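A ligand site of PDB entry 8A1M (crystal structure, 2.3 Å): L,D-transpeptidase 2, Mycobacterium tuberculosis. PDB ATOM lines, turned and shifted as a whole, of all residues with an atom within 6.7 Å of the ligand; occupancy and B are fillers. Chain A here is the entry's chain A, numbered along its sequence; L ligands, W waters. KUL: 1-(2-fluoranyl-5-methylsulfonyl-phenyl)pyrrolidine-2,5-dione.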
ATOM      1  N   GLY A 228     -12.765 -14.719  11.490  1.00  0.00           N
ATOM      2  CA  GLY A 228     -14.102 -14.187  11.269  1.00  0.00           C
ATOM      3  C   GLY A 228     -15.154 -14.993  12.015  1.00  0.00           C
ATOM      4  O   GLY A 228     -15.140 -16.226  12.004  1.00  0.00           O
ATOM      5  N   THR A 232     -19.688 -13.562   9.527  1.00  0.00           N
ATOM      6  CA  THR A 232     -18.745 -13.024   8.546  1.00  0.00           C
ATOM      7  C   THR A 232     -17.453 -13.820   8.648  1.00  0.00           C
ATOM      8  O   THR A 232     -16.414 -13.313   9.094  1.00  0.00           O
ATOM      9  CB  THR A 232     -18.502 -11.538   8.760  1.00  0.00           C
ATOM     10  OG1 THR A 232     -18.040 -11.317  10.103  1.00  0.00           O
ATOM     11  CG2 THR A 232     -19.786 -10.745   8.544  1.00  0.00           C
ATOM     12  N   PRO A 233     -17.478 -15.082   8.216  1.00  0.00           N
ATOM     13  CA  PRO A 233     -16.343 -15.967   8.468  1.00  0.00           C
ATOM     14  C   PRO A 233     -15.176 -15.718   7.521  1.00  0.00           C
ATOM     15  O   PRO A 233     -15.319 -15.161   6.431  1.00  0.00           O
ATOM     16  CB  PRO A 233     -16.937 -17.362   8.239  1.00  0.00           C
ATOM     17  CG  PRO A 233     -17.981 -17.136   7.204  1.00  0.00           C
ATOM     18  CD  PRO A 233     -18.547 -15.763   7.477  1.00  0.00           C
ATOM     19  N   THR A 234     -14.002 -16.161   7.968  1.00  0.00           N
ATOM     20  CA  THR A 234     -12.836 -16.217   7.109  1.00  0.00           C
ATOM     21  C   THR A 234     -12.952 -17.418   6.185  1.00  0.00           C
ATOM     22  O   THR A 234     -13.234 -18.530   6.632  1.00  0.00           O
ATOM     23  CB  THR A 234     -11.559 -16.303   7.936  1.00  0.00           C
ATOM     24  OG1 THR A 234     -11.533 -15.235   8.897  1.00  0.00           O
ATOM     25  CG2 THR A 234     -10.327 -16.200   7.036  1.00  0.00           C
ATOM     26  N   MET A 250      -8.403   0.826   8.332  1.00  0.00           N
ATOM     27  CA  MET A 250      -9.383  -0.036   7.673  1.00  0.00           C
ATOM     28  C   MET A 250     -10.686   0.727   7.521  1.00  0.00           C
ATOM     29  O   MET A 250     -11.223   1.246   8.509  1.00  0.00           O
ATOM     30  CB  MET A 250      -9.609  -1.311   8.482  1.00  0.00           C
ATOM     31  CG  MET A 250      -8.372  -2.167   8.661  1.00  0.00           C
ATOM     32  SD  MET A 250      -7.622  -2.650   7.109  1.00  0.00           S
ATOM     33  CE  MET A 250      -6.137  -3.456   7.707  1.00  0.00           C
ATOM     34  N   ASP A 251     -11.212   0.811   6.295  1.00  0.00           N
ATOM     35  CA  ASP A 251     -12.433   1.557   6.027  1.00  0.00           C
ATOM     36  C   ASP A 251     -13.325   0.680   5.160  1.00  0.00           C
ATOM     37  O   ASP A 251     -12.976   0.405   4.014  1.00  0.00           O
ATOM     38  CB  ASP A 251     -12.112   2.889   5.317  1.00  0.00           C
ATOM     39  CG  ASP A 251     -13.351   3.735   5.053  1.00  0.00           C
ATOM     40  OD1 ASP A 251     -14.471   3.216   5.097  1.00  0.00           O
ATOM     41  OD2 ASP A 251     -13.180   4.951   4.775  1.00  0.00           O
ATOM     42  N   SER A 252     -14.477   0.274   5.696  1.00  0.00           N
ATOM     43  CA  SER A 252     -15.376  -0.618   4.970  1.00  0.00           C
ATOM     44  C   SER A 252     -15.950   0.009   3.714  1.00  0.00           C
ATOM     45  O   SER A 252     -16.421  -0.716   2.831  1.00  0.00           O
ATOM     46  CB  SER A 252     -16.510  -1.043   5.893  1.00  0.00           C
ATOM     47  OG  SER A 252     -17.471  -0.013   6.001  1.00  0.00           O
ATOM     48  N   THR A 254     -14.515   1.319   1.286  1.00  0.00           N
ATOM     49  CA  THR A 254     -13.744   0.981   0.102  1.00  0.00           C
ATOM     50  C   THR A 254     -14.318  -0.231  -0.638  1.00  0.00           C
ATOM     51  O   THR A 254     -13.900  -0.496  -1.769  1.00  0.00           O
ATOM     52  CB  THR A 254     -12.283   0.721   0.466  1.00  0.00           C
ATOM     53  OG1 THR A 254     -12.186  -0.435   1.311  1.00  0.00           O
ATOM     54  CG2 THR A 254     -11.685   1.923   1.182  1.00  0.00           C
ATOM     55  N   TYR A 255     -15.241  -0.970  -0.016  1.00  0.00           N
ATOM     56  CA  TYR A 255     -15.886  -2.120  -0.638  1.00  0.00           C
ATOM     57  C   TYR A 255     -17.380  -1.888  -0.875  1.00  0.00           C
ATOM     58  O   TYR A 255     -18.090  -2.844  -1.192  1.00  0.00           O
ATOM     59  CB  TYR A 255     -15.692  -3.364   0.218  1.00  0.00           C
ATOM     60  CG  TYR A 255     -14.256  -3.728   0.473  1.00  0.00           C
ATOM     61  CD1 TYR A 255     -13.573  -4.586  -0.380  1.00  0.00           C
ATOM     62  CD2 TYR A 255     -13.575  -3.224   1.572  1.00  0.00           C
ATOM     63  CE1 TYR A 255     -12.252  -4.924  -0.152  1.00  0.00           C
ATOM     64  CE2 TYR A 255     -12.256  -3.554   1.812  1.00  0.00           C
ATOM     65  CZ  TYR A 255     -11.604  -4.406   0.950  1.00  0.00           C
ATOM     66  OH  TYR A 255     -10.285  -4.734   1.181  1.00  0.00           O
ATOM     67  N   GLY A 256     -17.859  -0.666  -0.731  1.00  0.00           N
ATOM     68  CA  GLY A 256     -19.268  -0.371  -0.900  1.00  0.00           C
ATOM     69  C   GLY A 256     -20.110  -0.553   0.338  1.00  0.00           C
ATOM     70  O   GLY A 256     -21.331  -0.371   0.268  1.00  0.00           O
ATOM     71  N   VAL A 257     -19.504  -0.924   1.473  1.00  0.00           N
ATOM     72  CA  VAL A 257     -20.223  -1.118   2.731  1.00  0.00           C
ATOM     73  C   VAL A 257     -20.118   0.186   3.526  1.00  0.00           C
ATOM     74  O   VAL A 257     -19.016   0.503   4.029  1.00  0.00           O
ATOM     75  CB  VAL A 257     -19.651  -2.293   3.529  1.00  0.00           C
ATOM     76  CG1 VAL A 257     -20.507  -2.559   4.756  1.00  0.00           C
ATOM     77  CG2 VAL A 257     -19.558  -3.538   2.660  1.00  0.00           C
ATOM     78  N   ASN A 263     -22.850  -3.380   9.724  1.00  0.00           N
ATOM     79  CA  ASN A 263     -21.706  -4.203   9.352  1.00  0.00           C
ATOM     80  C   ASN A 263     -20.540  -3.375   8.819  1.00  0.00           C
ATOM     81  O   ASN A 263     -19.555  -3.961   8.339  1.00  0.00           O
ATOM     82  CB  ASN A 263     -22.129  -5.246   8.308  1.00  0.00           C
ATOM     83  CG  ASN A 263     -21.733  -6.651   8.704  1.00  0.00           C
ATOM     84  OD1 ASN A 263     -22.535  -7.580   8.630  1.00  0.00           O
ATOM     85  ND2 ASN A 263     -20.486  -6.823   9.137  1.00  0.00           N
ATOM     86  N   GLY A 264     -20.624  -2.051   8.873  1.00  0.00           N
ATOM     87  CA  GLY A 264     -19.521  -1.207   8.477  1.00  0.00           C
ATOM     88  C   GLY A 264     -18.504  -1.041   9.601  1.00  0.00           C
ATOM     89  O   GLY A 264     -18.666  -1.548  10.708  1.00  0.00           O
ATOM     90  N   TYR A 265     -17.433  -0.328   9.285  1.00  0.00           N
ATOM     91  CA  TYR A 265     -16.372  -0.127  10.263  1.00  0.00           C
ATOM     92  C   TYR A 265     -15.389   0.914   9.739  1.00  0.00           C
ATOM     93  O   TYR A 265     -15.255   1.116   8.524  1.00  0.00           O
ATOM     94  CB  TYR A 265     -15.631  -1.439  10.565  1.00  0.00           C
ATOM     95  CG  TYR A 265     -15.115  -2.141   9.325  1.00  0.00           C
ATOM     96  CD1 TYR A 265     -15.787  -3.222   8.782  1.00  0.00           C
ATOM     97  CD2 TYR A 265     -13.951  -1.711   8.702  1.00  0.00           C
ATOM     98  CE1 TYR A 265     -15.321  -3.853   7.642  1.00  0.00           C
ATOM     99  CE2 TYR A 265     -13.478  -2.331   7.565  1.00  0.00           C
ATOM    100  CZ  TYR A 265     -14.162  -3.409   7.043  1.00  0.00           C
ATOM    101  OH  TYR A 265     -13.688  -4.029   5.905  1.00  0.00           O
ATOM    102  N   VAL A 269      -5.338   0.310  12.632  1.00  0.00           N
ATOM    103  CA  VAL A 269      -4.718  -0.905  13.122  1.00  0.00           C
ATOM    104  C   VAL A 269      -3.231  -0.888  12.772  1.00  0.00           C
ATOM    105  O   VAL A 269      -2.807  -0.204  11.839  1.00  0.00           O
ATOM    106  CB  VAL A 269      -5.384  -2.180  12.561  1.00  0.00           C
ATOM    107  CG1 VAL A 269      -6.898  -2.085  12.691  1.00  0.00           C
ATOM    108  CG2 VAL A 269      -4.963  -2.409  11.119  1.00  0.00           C
ATOM    109  N   SER A 276      -5.785 -10.773   1.104  1.00  0.00           N
ATOM    110  CA  SER A 276      -6.871 -10.899   0.144  1.00  0.00           C
ATOM    111  C   SER A 276      -7.345  -9.507  -0.266  1.00  0.00           C
ATOM    112  O   SER A 276      -7.385  -8.587   0.563  1.00  0.00           O
ATOM    113  CB  SER A 276      -8.045 -11.694   0.706  1.00  0.00           C
ATOM    114  OG  SER A 276      -9.051 -10.835   1.213  1.00  0.00           O
ATOM    115  N   SER A 278     -10.368  -8.841  -0.949  1.00  0.00           N
ATOM    116  CA  SER A 278     -11.642  -8.632  -0.281  1.00  0.00           C
ATOM    117  C   SER A 278     -11.491  -8.069   1.122  1.00  0.00           C
ATOM    118  O   SER A 278     -12.507  -7.756   1.749  1.00  0.00           O
ATOM    119  CB  SER A 278     -12.430  -9.956  -0.238  1.00  0.00           C
ATOM    120  OG  SER A 278     -11.693 -10.976   0.406  1.00  0.00           O
ATOM    121  N   GLY A 279     -10.276  -7.929   1.624  1.00  0.00           N
ATOM    122  CA  GLY A 279     -10.013  -7.249   2.862  1.00  0.00           C
ATOM    123  C   GLY A 279      -9.514  -8.098   4.019  1.00  0.00           C
ATOM    124  O   GLY A 279      -9.580  -7.650   5.162  1.00  0.00           O
ATOM    125  N   VAL A 280      -9.019  -9.308   3.754  1.00  0.00           N
ATOM    126  CA  VAL A 280      -8.496 -10.150   4.821  1.00  0.00           C
ATOM    127  C   VAL A 280      -7.051  -9.740   5.095  1.00  0.00           C
ATOM    128  O   VAL A 280      -6.216  -9.747   4.191  1.00  0.00           O
ATOM    129  CB  VAL A 280      -8.606 -11.637   4.464  1.00  0.00           C
ATOM    130  CG1 VAL A 280      -8.062 -12.500   5.588  1.00  0.00           C
ATOM    131  CG2 VAL A 280     -10.048 -12.000   4.170  1.00  0.00           C
ATOM    132  N   PHE A 281      -6.771  -9.376   6.348  1.00  0.00           N
ATOM    133  CA  PHE A 281      -5.445  -8.989   6.790  1.00  0.00           C
ATOM    134  C   PHE A 281      -5.049  -9.802   8.016  1.00  0.00           C
ATOM    135  O   PHE A 281      -5.900 -10.311   8.748  1.00  0.00           O
ATOM    136  CB  PHE A 281      -5.386  -7.506   7.165  1.00  0.00           C
ATOM    137  CG  PHE A 281      -5.381  -6.562   5.990  1.00  0.00           C
ATOM    138  CD1 PHE A 281      -4.226  -5.906   5.630  1.00  0.00           C
ATOM    139  CD2 PHE A 281      -6.538  -6.333   5.273  1.00  0.00           C
ATOM    140  CE1 PHE A 281      -4.214  -5.039   4.559  1.00  0.00           C
ATOM    141  CE2 PHE A 281      -6.536  -5.468   4.201  1.00  0.00           C
ATOM    142  CZ  PHE A 281      -5.371  -4.812   3.852  1.00  0.00           C
ATOM    143  N   HIS A 283      -3.318  -8.626  11.274  1.00  0.00           N
ATOM    144  CA  HIS A 283      -3.025  -7.336  11.893  1.00  0.00           C
ATOM    145  C   HIS A 283      -3.028  -7.473  13.416  1.00  0.00           C
ATOM    146  O   HIS A 283      -3.437  -8.492  13.977  1.00  0.00           O
ATOM    147  CB  HIS A 283      -4.030  -6.263  11.454  1.00  0.00           C
ATOM    148  CG  HIS A 283      -5.406  -6.498  11.967  1.00  0.00           C
ATOM    149  ND1 HIS A 283      -5.839  -6.018  13.194  1.00  0.00           N
ATOM    150  CD2 HIS A 283      -6.463  -7.154  11.431  1.00  0.00           C
ATOM    151  CE1 HIS A 283      -7.101  -6.370  13.381  1.00  0.00           C
ATOM    152  NE2 HIS A 283      -7.506  -7.062  12.332  1.00  0.00           N
ATOM    153  N   SER A 298     -14.106 -11.428  14.316  1.00  0.00           N
ATOM    154  CA  SER A 298     -13.786 -10.388  13.346  1.00  0.00           C
ATOM    155  C   SER A 298     -14.681 -10.511  12.102  1.00  0.00           C
ATOM    156  O   SER A 298     -15.585 -11.341  12.051  1.00  0.00           O
ATOM    157  CB  SER A 298     -12.311 -10.460  12.964  1.00  0.00           C
ATOM    158  OG  SER A 298     -12.079 -11.505  12.034  1.00  0.00           O
ATOM    159  N   HIS A 299     -14.406  -9.662  11.104  1.00  0.00           N
ATOM    160  CA  HIS A 299     -15.107  -9.714   9.819  1.00  0.00           C
ATOM    161  C   HIS A 299     -14.340 -10.519   8.775  1.00  0.00           C
ATOM    162  O   HIS A 299     -14.648 -10.422   7.587  1.00  0.00           O
ATOM    163  CB  HIS A 299     -15.351  -8.305   9.273  1.00  0.00           C
ATOM    164  CG  HIS A 299     -15.919  -7.343  10.268  1.00  0.00           C
ATOM    165  ND1 HIS A 299     -17.206  -6.853  10.171  1.00  0.00           N
ATOM    166  CD2 HIS A 299     -15.375  -6.761  11.363  1.00  0.00           C
ATOM    167  CE1 HIS A 299     -17.436  -6.014  11.173  1.00  0.00           C
ATOM    168  NE2 HIS A 299     -16.335  -5.946  11.912  1.00  0.00           N
ATOM    169  N   GLY A 300     -13.337 -11.301   9.184  1.00  0.00           N
ATOM    170  CA  GLY A 300     -12.532 -12.074   8.252  1.00  0.00           C
ATOM    171  C   GLY A 300     -11.053 -11.963   8.534  1.00  0.00           C
ATOM    172  O   GLY A 300     -10.293 -12.900   8.271  1.00  0.00           O
ATOM    173  N   CYS A 301     -10.647 -10.817   9.068  1.00  0.00           N
ATOM    174  CA  CYS A 301      -9.244 -10.563   9.344  1.00  0.00           C
ATOM    175  C   CYS A 301      -8.714 -11.500  10.417  1.00  0.00           C
ATOM    176  O   CYS A 301      -9.360 -11.763  11.381  1.00  0.00           O
ATOM    177  CB  CYS A 301      -9.093  -9.119   9.824  1.00  0.00           C
ATOM    178  SG  CYS A 301      -8.855  -8.023   8.393  1.00  0.00           S
ATOM    179  N   LEU A 302      -7.499 -11.993  10.213  1.00  0.00           N
ATOM    180  CA  LEU A 302      -6.831 -12.821  11.213  1.00  0.00           C
ATOM    181  C   LEU A 302      -6.250 -11.938  12.313  1.00  0.00           C
ATOM    182  O   LEU A 302      -5.173 -11.371  12.166  1.00  0.00           O
ATOM    183  CB  LEU A 302      -5.736 -13.669  10.566  1.00  0.00           C
ATOM    184  CG  LEU A 302      -6.183 -15.032  10.028  1.00  0.00           C
ATOM    185  CD1 LEU A 302      -7.431 -14.921   9.166  1.00  0.00           C
ATOM    186  CD2 LEU A 302      -5.051 -15.703   9.251  1.00  0.00           C
ATOM    187  N   ASN A 303      -6.998 -11.803  13.405  1.00  0.00           N
ATOM    188  CA  ASN A 303      -6.546 -11.009  14.543  1.00  0.00           C
ATOM    189  C   ASN A 303      -5.459 -11.756  15.303  1.00  0.00           C
ATOM    190  O   ASN A 303      -5.607 -12.946  15.619  1.00  0.00           O
ATOM    191  CB  ASN A 303      -7.712 -10.707  15.473  1.00  0.00           C
ATOM    192  CG  ASN A 303      -8.705  -9.746  14.862  1.00  0.00           C
ATOM    193  OD1 ASN A 303      -8.429  -9.112  13.840  1.00  0.00           O
ATOM    194  ND2 ASN A 303      -9.871  -9.614  15.502  1.00  0.00           N
HETATM  195  C10 KUL L   1      -9.703  -6.447   8.506  1.00  0.00           C
HETATM  196  C20 KUL L   1     -12.256  -9.008   5.977  1.00  0.00           C
HETATM  197  C22 KUL L   1     -13.049  -9.546   4.970  1.00  0.00           C
HETATM  198  C01 KUL L   1     -15.218  -5.329   3.187  1.00  0.00           C
HETATM  199  C04 KUL L   1     -14.384  -7.560   4.981  1.00  0.00           C
HETATM  200  C05 KUL L   1     -13.589  -7.031   5.986  1.00  0.00           C
HETATM  201  C06 KUL L   1     -12.521  -7.749   6.485  1.00  0.00           C
HETATM  202  C08 KUL L   1     -11.755  -7.337   9.037  1.00  0.00           C
HETATM  203  C09 KUL L   1     -10.706  -6.482   9.613  1.00  0.00           C
HETATM  204  C18 KUL L   1     -10.647  -6.213   7.309  1.00  0.00           C
HETATM  205  C23 KUL L   1     -14.119  -8.819   4.473  1.00  0.00           C
HETATM  206  F21 KUL L   1     -11.206  -9.734   6.453  1.00  0.00           F
HETATM  207  N07 KUL L   1     -11.701  -7.153   7.538  1.00  0.00           N
HETATM  208  O03 KUL L   1     -16.565  -6.000   5.437  1.00  0.00           O
HETATM  209  O17 KUL L   1     -12.479  -8.044   9.650  1.00  0.00           O
HETATM  210  O19 KUL L   1     -10.544  -5.455   6.409  1.00  0.00           O
HETATM  211  O24 KUL L   1     -16.784  -7.464   3.713  1.00  0.00           O
HETATM  212  S02 KUL L   1     -15.792  -6.604   4.350  1.00  0.00           S
HETATM  213  O   HOH W   1     -18.091  -7.569   7.478  1.00  0.00           O
HETATM  214  O   HOH W   2     -15.280  -8.024   0.969  1.00  0.00           O
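The backbone NH (N) of Gly 279 sits close to the side-chain hydroxyl (OH) of Tyr 255, at 3.2 Å. The backbone NH of Gly 300 is in hydrogen-bond range of the side-chain hydroxyl of Ser 298, 3.1 Å away. The side-chain hydroxyl (OG) of Ser 278 sits at hydrogen-bond distance from the side-chain hydroxyl (OG) of Ser 276 (2.8 Å). N of Ser 252 is in hydrogen-bond range of O of Tyr 265 (3.1 Å). The backbone NH (N) of Val 280 sits at hydrogen-bond distance from the side-chain hydroxyl (OG) of Ser 276, at 3.0 Å. The backbone carbonyl oxygen (O) of Gly 300 lies within hydrogen-bond range of the side-chain hydroxyl (OG1) of Thr 234 (2.7 Å). OG of Ser 276 sits at hydrogen-bond distance from N of Gly 279 (3.2 Å). SG of Cys 301 lies within hydrogen-bond range of N of Phe 281, at 3.2 Å.
OH of Tyr 265 sits close to O19 of the ligand (3.5 Å). The backbone carbonyl oxygen (O) of Gly 279 sits close to an oxygen (O19) of the ligand (2.7 Å). N of His 299 sits at hydrogen-bond distance from O17 of the ligand, at 2.9 Å. The side-chain sulfur (SG) of Cys 301 is bonded to a carbon (C10) of the ligand. The backbone NH (N) of Cys 301 is in hydrogen-bond range of an oxygen (O17) of the ligand, 3.4 Å away. The backbone NH of Gly 300 lies within hydrogen-bond range of an oxygen (O17) of the ligand (3.4 Å).
F21 of the ligand lies close to N of Val 280 (3.5 Å). Tyr 255 touches the ligand. O of Ser 278 touches C23 of the ligand, at 3.3 Å. Hydrophobic or aromatic side chains within 4 Å of the ligand: Tyr 255, Tyr 265, Val 280 and His 299. Eight residues have an atom within 4 Å of the ligand: Tyr 255, Tyr 265, Ser 278, Gly 279, Val 280, His 299, Gly 300 and Cys 301. The nearest printed residue that does not touch the ligand is Ser 298 (4.1 Å).
Water W1 lies within hydrogen-bond range of a ring nitrogen (ND1) of His 299 (2.9 Å), an oxygen (O03) of the ligand (3.0 Å) and the side-chain amide nitrogen (ND2) of Asn 263 (3.0 Å). Water W2 bridges O of Ser 278 (2.9 Å) and O24 of the ligand (3.2 Å).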
